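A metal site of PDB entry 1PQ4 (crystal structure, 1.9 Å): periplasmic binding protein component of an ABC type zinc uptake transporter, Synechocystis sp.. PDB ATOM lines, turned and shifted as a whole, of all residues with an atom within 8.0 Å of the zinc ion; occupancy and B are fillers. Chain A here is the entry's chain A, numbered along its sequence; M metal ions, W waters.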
ATOM      1  N   ASP A  35      32.302 -11.789 -11.740  1.00  0.00           N
ATOM      2  CA  ASP A  35      31.976 -10.684 -10.836  1.00  0.00           C
ATOM      3  C   ASP A  35      31.169  -9.722 -11.733  1.00  0.00           C
ATOM      4  O   ASP A  35      31.725  -9.142 -12.682  1.00  0.00           O
ATOM      5  CB  ASP A  35      33.260 -10.031 -10.311  1.00  0.00           C
ATOM      6  CG  ASP A  35      33.031  -8.620  -9.746  1.00  0.00           C
ATOM      7  OD1 ASP A  35      31.857  -8.236  -9.451  1.00  0.00           O
ATOM      8  OD2 ASP A  35      34.023  -7.892  -9.580  1.00  0.00           O
ATOM      9  N   PRO A  36      29.864  -9.530 -11.447  1.00  0.00           N
ATOM     10  CA  PRO A  36      29.010  -8.645 -12.249  1.00  0.00           C
ATOM     11  C   PRO A  36      29.434  -7.188 -12.198  1.00  0.00           C
ATOM     12  O   PRO A  36      29.210  -6.444 -13.144  1.00  0.00           O
ATOM     13  CB  PRO A  36      27.607  -8.855 -11.650  1.00  0.00           C
ATOM     14  CG  PRO A  36      27.903  -9.117 -10.210  1.00  0.00           C
ATOM     15  CD  PRO A  36      29.137  -9.994 -10.237  1.00  0.00           C
ATOM     16  N   HIS A  37      30.045  -6.788 -11.092  1.00  0.00           N
ATOM     17  CA  HIS A  37      30.489  -5.419 -10.948  1.00  0.00           C
ATOM     18  C   HIS A  37      31.626  -4.962 -11.884  1.00  0.00           C
ATOM     19  O   HIS A  37      31.851  -3.776 -12.043  1.00  0.00           O
ATOM     20  CB  HIS A  37      30.895  -5.174  -9.502  1.00  0.00           C
ATOM     21  CG  HIS A  37      29.829  -5.542  -8.514  1.00  0.00           C
ATOM     22  ND1 HIS A  37      28.728  -4.759  -8.283  1.00  0.00           N
ATOM     23  CD2 HIS A  37      29.707  -6.621  -7.706  1.00  0.00           C
ATOM     24  CE1 HIS A  37      27.965  -5.328  -7.364  1.00  0.00           C
ATOM     25  NE2 HIS A  37      28.539  -6.457  -6.995  1.00  0.00           N
ATOM     26  N   PHE A  62      23.192  -0.609 -11.074  1.00  0.00           N
ATOM     27  CA  PHE A  62      23.909  -1.877 -11.336  1.00  0.00           C
ATOM     28  C   PHE A  62      24.483  -1.971 -12.767  1.00  0.00           C
ATOM     29  O   PHE A  62      25.598  -2.449 -12.963  1.00  0.00           O
ATOM     30  CB  PHE A  62      22.963  -3.052 -11.120  1.00  0.00           C
ATOM     31  CG  PHE A  62      23.643  -4.376 -11.169  1.00  0.00           C
ATOM     32  CD1 PHE A  62      24.515  -4.754 -10.163  1.00  0.00           C
ATOM     33  CD2 PHE A  62      23.341  -5.276 -12.162  1.00  0.00           C
ATOM     34  CE1 PHE A  62      25.069  -6.037 -10.117  1.00  0.00           C
ATOM     35  CE2 PHE A  62      23.899  -6.582 -12.135  1.00  0.00           C
ATOM     36  CZ  PHE A  62      24.748  -6.961 -11.101  1.00  0.00           C
ATOM     37  N   MET A  91      25.820   2.029   0.162  1.00  0.00           N
ATOM     38  CA  MET A  91      27.086   1.362   0.411  1.00  0.00           C
ATOM     39  C   MET A  91      28.033   2.525   0.694  1.00  0.00           C
ATOM     40  O   MET A  91      28.569   3.143  -0.240  1.00  0.00           O
ATOM     41  CB  MET A  91      27.576   0.595  -0.807  1.00  0.00           C
ATOM     42  CG  MET A  91      26.822  -0.678  -1.088  1.00  0.00           C
ATOM     43  SD  MET A  91      27.636  -1.703  -2.350  1.00  0.00           S
ATOM     44  CE  MET A  91      27.365  -0.676  -3.860  1.00  0.00           C
ATOM     45  N   ASP A 131      23.028   0.404  -2.736  1.00  0.00           N
ATOM     46  CA  ASP A 131      23.478  -0.993  -2.735  1.00  0.00           C
ATOM     47  C   ASP A 131      22.534  -1.640  -3.721  1.00  0.00           C
ATOM     48  O   ASP A 131      21.326  -1.637  -3.532  1.00  0.00           O
ATOM     49  CB  ASP A 131      23.260  -1.606  -1.357  1.00  0.00           C
ATOM     50  CG  ASP A 131      23.800  -3.028  -1.260  1.00  0.00           C
ATOM     51  OD1 ASP A 131      23.750  -3.776  -2.265  1.00  0.00           O
ATOM     52  OD2 ASP A 131      24.260  -3.370  -0.171  1.00  0.00           O
ATOM     53  N   PRO A 132      23.077  -2.239  -4.781  1.00  0.00           N
ATOM     54  CA  PRO A 132      22.191  -2.840  -5.776  1.00  0.00           C
ATOM     55  C   PRO A 132      21.750  -4.312  -5.563  1.00  0.00           C
ATOM     56  O   PRO A 132      21.003  -4.822  -6.368  1.00  0.00           O
ATOM     57  CB  PRO A 132      23.033  -2.723  -7.051  1.00  0.00           C
ATOM     58  CG  PRO A 132      24.404  -3.086  -6.542  1.00  0.00           C
ATOM     59  CD  PRO A 132      24.496  -2.374  -5.172  1.00  0.00           C
ATOM     60  N   HIS A 133      22.151  -4.916  -4.461  1.00  0.00           N
ATOM     61  CA  HIS A 133      21.893  -6.343  -4.290  1.00  0.00           C
ATOM     62  C   HIS A 133      20.490  -6.681  -3.853  1.00  0.00           C
ATOM     63  O   HIS A 133      20.258  -7.483  -2.929  1.00  0.00           O
ATOM     64  CB  HIS A 133      22.955  -6.893  -3.335  1.00  0.00           C
ATOM     65  CG  HIS A 133      24.363  -6.684  -3.806  1.00  0.00           C
ATOM     66  ND1 HIS A 133      25.128  -5.595  -3.430  1.00  0.00           N
ATOM     67  CD2 HIS A 133      25.159  -7.448  -4.599  1.00  0.00           C
ATOM     68  CE1 HIS A 133      26.331  -5.695  -3.959  1.00  0.00           C
ATOM     69  NE2 HIS A 133      26.380  -6.809  -4.665  1.00  0.00           N
ATOM     70  N   TRP A 135      18.244  -8.354  -5.317  1.00  0.00           N
ATOM     71  CA  TRP A 135      17.651  -9.611  -5.785  1.00  0.00           C
ATOM     72  C   TRP A 135      17.758 -10.744  -4.782  1.00  0.00           C
ATOM     73  O   TRP A 135      17.290 -11.866  -5.050  1.00  0.00           O
ATOM     74  CB  TRP A 135      18.271 -10.039  -7.139  1.00  0.00           C
ATOM     75  CG  TRP A 135      19.746 -10.449  -7.005  1.00  0.00           C
ATOM     76  CD1 TRP A 135      20.248 -11.692  -6.720  1.00  0.00           C
ATOM     77  CD2 TRP A 135      20.862  -9.590  -7.215  1.00  0.00           C
ATOM     78  NE1 TRP A 135      21.640 -11.658  -6.738  1.00  0.00           N
ATOM     79  CE2 TRP A 135      22.035 -10.379  -7.047  1.00  0.00           C
ATOM     80  CE3 TRP A 135      20.998  -8.225  -7.544  1.00  0.00           C
ATOM     81  CZ2 TRP A 135      23.325  -9.837  -7.188  1.00  0.00           C
ATOM     82  CZ3 TRP A 135      22.267  -7.691  -7.681  1.00  0.00           C
ATOM     83  CH2 TRP A 135      23.422  -8.502  -7.521  1.00  0.00           C
ATOM     84  N   LEU A 136      18.396 -10.458  -3.644  1.00  0.00           N
ATOM     85  CA  LEU A 136      18.556 -11.506  -2.636  1.00  0.00           C
ATOM     86  C   LEU A 136      17.617 -11.327  -1.452  1.00  0.00           C
ATOM     87  O   LEU A 136      17.776 -11.955  -0.424  1.00  0.00           O
ATOM     88  CB  LEU A 136      20.033 -11.569  -2.175  1.00  0.00           C
ATOM     89  CG  LEU A 136      20.917 -12.041  -3.355  1.00  0.00           C
ATOM     90  CD1 LEU A 136      22.375 -11.719  -3.041  1.00  0.00           C
ATOM     91  CD2 LEU A 136      20.737 -13.531  -3.656  1.00  0.00           C
ATOM     92  N   HIS A 197      32.543 -10.811  -0.233  1.00  0.00           N
ATOM     93  CA  HIS A 197      31.903  -9.691  -0.967  1.00  0.00           C
ATOM     94  C   HIS A 197      30.523  -9.437  -0.348  1.00  0.00           C
ATOM     95  O   HIS A 197      29.715 -10.366  -0.218  1.00  0.00           O
ATOM     96  CB  HIS A 197      31.790 -10.093  -2.426  1.00  0.00           C
ATOM     97  CG  HIS A 197      31.021  -9.132  -3.252  1.00  0.00           C
ATOM     98  ND1 HIS A 197      31.537  -7.908  -3.640  1.00  0.00           N
ATOM     99  CD2 HIS A 197      29.774  -9.200  -3.786  1.00  0.00           C
ATOM    100  CE1 HIS A 197      30.647  -7.269  -4.380  1.00  0.00           C
ATOM    101  NE2 HIS A 197      29.569  -8.031  -4.478  1.00  0.00           N
ATOM    102  N   PRO A 198      30.242  -8.176   0.038  1.00  0.00           N
ATOM    103  CA  PRO A 198      28.977  -7.832   0.672  1.00  0.00           C
ATOM    104  C   PRO A 198      27.794  -7.789  -0.260  1.00  0.00           C
ATOM    105  O   PRO A 198      27.339  -6.728  -0.663  1.00  0.00           O
ATOM    106  CB  PRO A 198      29.278  -6.481   1.351  1.00  0.00           C
ATOM    107  CG  PRO A 198      30.192  -5.826   0.350  1.00  0.00           C
ATOM    108  CD  PRO A 198      31.084  -6.984  -0.158  1.00  0.00           C
ATOM    109  N   SER A 199      27.301  -8.926  -0.641  1.00  0.00           N
ATOM    110  CA  SER A 199      26.122  -8.848  -1.489  1.00  0.00           C
ATOM    111  C   SER A 199      24.869  -9.166  -0.682  1.00  0.00           C
ATOM    112  O   SER A 199      23.779  -9.272  -1.245  1.00  0.00           O
ATOM    113  CB  SER A 199      26.267  -9.860  -2.622  1.00  0.00           C
ATOM    114  OG  SER A 199      26.705 -11.064  -2.117  1.00  0.00           O
ATOM    115  N   TRP A 200      25.008  -9.311   0.632  1.00  0.00           N
ATOM    116  CA  TRP A 200      23.860  -9.771   1.427  1.00  0.00           C
ATOM    117  C   TRP A 200      23.240  -8.742   2.371  1.00  0.00           C
ATOM    118  O   TRP A 200      22.558  -9.134   3.334  1.00  0.00           O
ATOM    119  CB  TRP A 200      24.262 -11.034   2.245  1.00  0.00           C
ATOM    120  CG  TRP A 200      24.923 -12.107   1.410  1.00  0.00           C
ATOM    121  CD1 TRP A 200      26.264 -12.263   1.152  1.00  0.00           C
ATOM    122  CD2 TRP A 200      24.253 -13.095   0.625  1.00  0.00           C
ATOM    123  NE1 TRP A 200      26.466 -13.287   0.248  1.00  0.00           N
ATOM    124  CE2 TRP A 200      25.236 -13.806  -0.093  1.00  0.00           C
ATOM    125  CE3 TRP A 200      22.896 -13.444   0.460  1.00  0.00           C
ATOM    126  CZ2 TRP A 200      24.923 -14.845  -0.972  1.00  0.00           C
ATOM    127  CZ3 TRP A 200      22.581 -14.476  -0.412  1.00  0.00           C
ATOM    128  CH2 TRP A 200      23.589 -15.168  -1.116  1.00  0.00           C
ATOM    129  N   GLU A 215      36.008  -7.811   2.010  1.00  0.00           N
ATOM    130  CA  GLU A 215      36.463  -6.859   0.990  1.00  0.00           C
ATOM    131  C   GLU A 215      36.183  -5.429   1.444  1.00  0.00           C
ATOM    132  O   GLU A 215      35.245  -5.177   2.182  1.00  0.00           O
ATOM    133  CB  GLU A 215      35.793  -7.106  -0.373  1.00  0.00           C
ATOM    134  CG  GLU A 215      34.363  -6.681  -0.468  1.00  0.00           C
ATOM    135  CD  GLU A 215      33.939  -6.268  -1.897  1.00  0.00           C
ATOM    136  OE1 GLU A 215      34.087  -7.072  -2.854  1.00  0.00           O
ATOM    137  OE2 GLU A 215      33.451  -5.110  -2.031  1.00  0.00           O
ATOM    138  N   GLU A 244      32.754 -16.303  -1.849  1.00  0.00           N
ATOM    139  CA  GLU A 244      31.797 -16.365  -2.935  1.00  0.00           C
ATOM    140  C   GLU A 244      32.525 -16.930  -4.149  1.00  0.00           C
ATOM    141  O   GLU A 244      33.725 -16.671  -4.321  1.00  0.00           O
ATOM    142  CB  GLU A 244      31.265 -14.947  -3.229  1.00  0.00           C
ATOM    143  CG  GLU A 244      30.099 -14.598  -2.391  1.00  0.00           C
ATOM    144  CD  GLU A 244      30.375 -13.513  -1.372  1.00  0.00           C
ATOM    145  OE1 GLU A 244      31.523 -13.440  -0.866  1.00  0.00           O
ATOM    146  OE2 GLU A 244      29.395 -12.755  -1.084  1.00  0.00           O
ATOM    147  N   GLN A 246      32.431 -16.164  -7.234  1.00  0.00           N
ATOM    148  CA  GLN A 246      32.901 -15.183  -8.221  1.00  0.00           C
ATOM    149  C   GLN A 246      34.125 -14.411  -7.788  1.00  0.00           C
ATOM    150  O   GLN A 246      34.649 -13.631  -8.558  1.00  0.00           O
ATOM    151  CB  GLN A 246      31.771 -14.191  -8.572  1.00  0.00           C
ATOM    152  CG  GLN A 246      30.539 -14.862  -9.188  1.00  0.00           C
ATOM    153  CD  GLN A 246      29.614 -15.518  -8.141  1.00  0.00           C
ATOM    154  OE1 GLN A 246      28.679 -16.266  -8.474  1.00  0.00           O
ATOM    155  NE2 GLN A 246      29.883 -15.220  -6.867  1.00  0.00           N
ATOM    156  N   PHE A 247      34.584 -14.601  -6.552  1.00  0.00           N
ATOM    157  CA  PHE A 247      35.754 -13.864  -6.090  1.00  0.00           C
ATOM    158  C   PHE A 247      36.728 -14.853  -5.481  1.00  0.00           C
ATOM    159  O   PHE A 247      36.361 -15.952  -5.097  1.00  0.00           O
ATOM    160  CB  PHE A 247      35.339 -12.833  -5.024  1.00  0.00           C
ATOM    161  CG  PHE A 247      34.239 -11.904  -5.466  1.00  0.00           C
ATOM    162  CD1 PHE A 247      32.906 -12.240  -5.298  1.00  0.00           C
ATOM    163  CD2 PHE A 247      34.540 -10.703  -6.096  1.00  0.00           C
ATOM    164  CE1 PHE A 247      31.889 -11.398  -5.743  1.00  0.00           C
ATOM    165  CE2 PHE A 247      33.522  -9.853  -6.551  1.00  0.00           C
ATOM    166  CZ  PHE A 247      32.205 -10.203  -6.377  1.00  0.00           C
ATOM    167  N   PRO A 268      25.879 -15.611  -4.681  1.00  0.00           N
ATOM    168  CA  PRO A 268      24.820 -14.590  -4.863  1.00  0.00           C
ATOM    169  C   PRO A 268      24.187 -14.609  -6.268  1.00  0.00           C
ATOM    170  O   PRO A 268      23.124 -14.029  -6.477  1.00  0.00           O
ATOM    171  CB  PRO A 268      25.545 -13.277  -4.557  1.00  0.00           C
ATOM    172  CG  PRO A 268      26.928 -13.543  -5.084  1.00  0.00           C
ATOM    173  CD  PRO A 268      27.216 -14.982  -4.539  1.00  0.00           C
ATOM    174  N   LEU A 269      24.827 -15.298  -7.231  1.00  0.00           N
ATOM    175  CA  LEU A 269      24.330 -15.321  -8.616  1.00  0.00           C
ATOM    176  C   LEU A 269      23.723 -16.642  -9.073  1.00  0.00           C
ATOM    177  O   LEU A 269      23.538 -16.860 -10.265  1.00  0.00           O
ATOM    178  CB  LEU A 269      25.433 -14.940  -9.642  1.00  0.00           C
ATOM    179  CG  LEU A 269      26.117 -13.584  -9.428  1.00  0.00           C
ATOM    180  CD1 LEU A 269      27.064 -13.281 -10.633  1.00  0.00           C
ATOM    181  CD2 LEU A 269      25.040 -12.491  -9.308  1.00  0.00           C
HETATM  182 ZN    ZN M   1      27.944  -7.781  -5.709  1.00  0.00          ZN
HETATM  183  O   HOH W   1      27.126  -9.763  -6.482  1.00  0.00           O
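OD1 of Asp 35 is in hydrogen-bond range of N of His 37. The side-chain carboxylate (OE1) of Glu 215 is in hydrogen-bond range of a ring nitrogen (ND1) of His 197, 2.8 Å away. N of His 197 sits at hydrogen-bond distance from OE1 of Glu 244, 2.9 Å away. The side-chain carboxylate (OD1) of Asp 131 is in hydrogen-bond range of a ring nitrogen (ND1) of His 133 (2.6 Å).
Of the 20 residues printed, 3 come within 4 Å of the zinc ion.
A ring nitrogen (NE2) of His 37 binds the zinc ion, at 1.9 Å. The zinc ion is bound by a ring nitrogen (NE2) of His 197 (2.1 Å). NE2 of His 133 is bound to the zinc ion, 2.1 Å away. The zinc ion is bound by water W1 (2.3 Å). The zinc ion has four donor atoms within binding distance.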
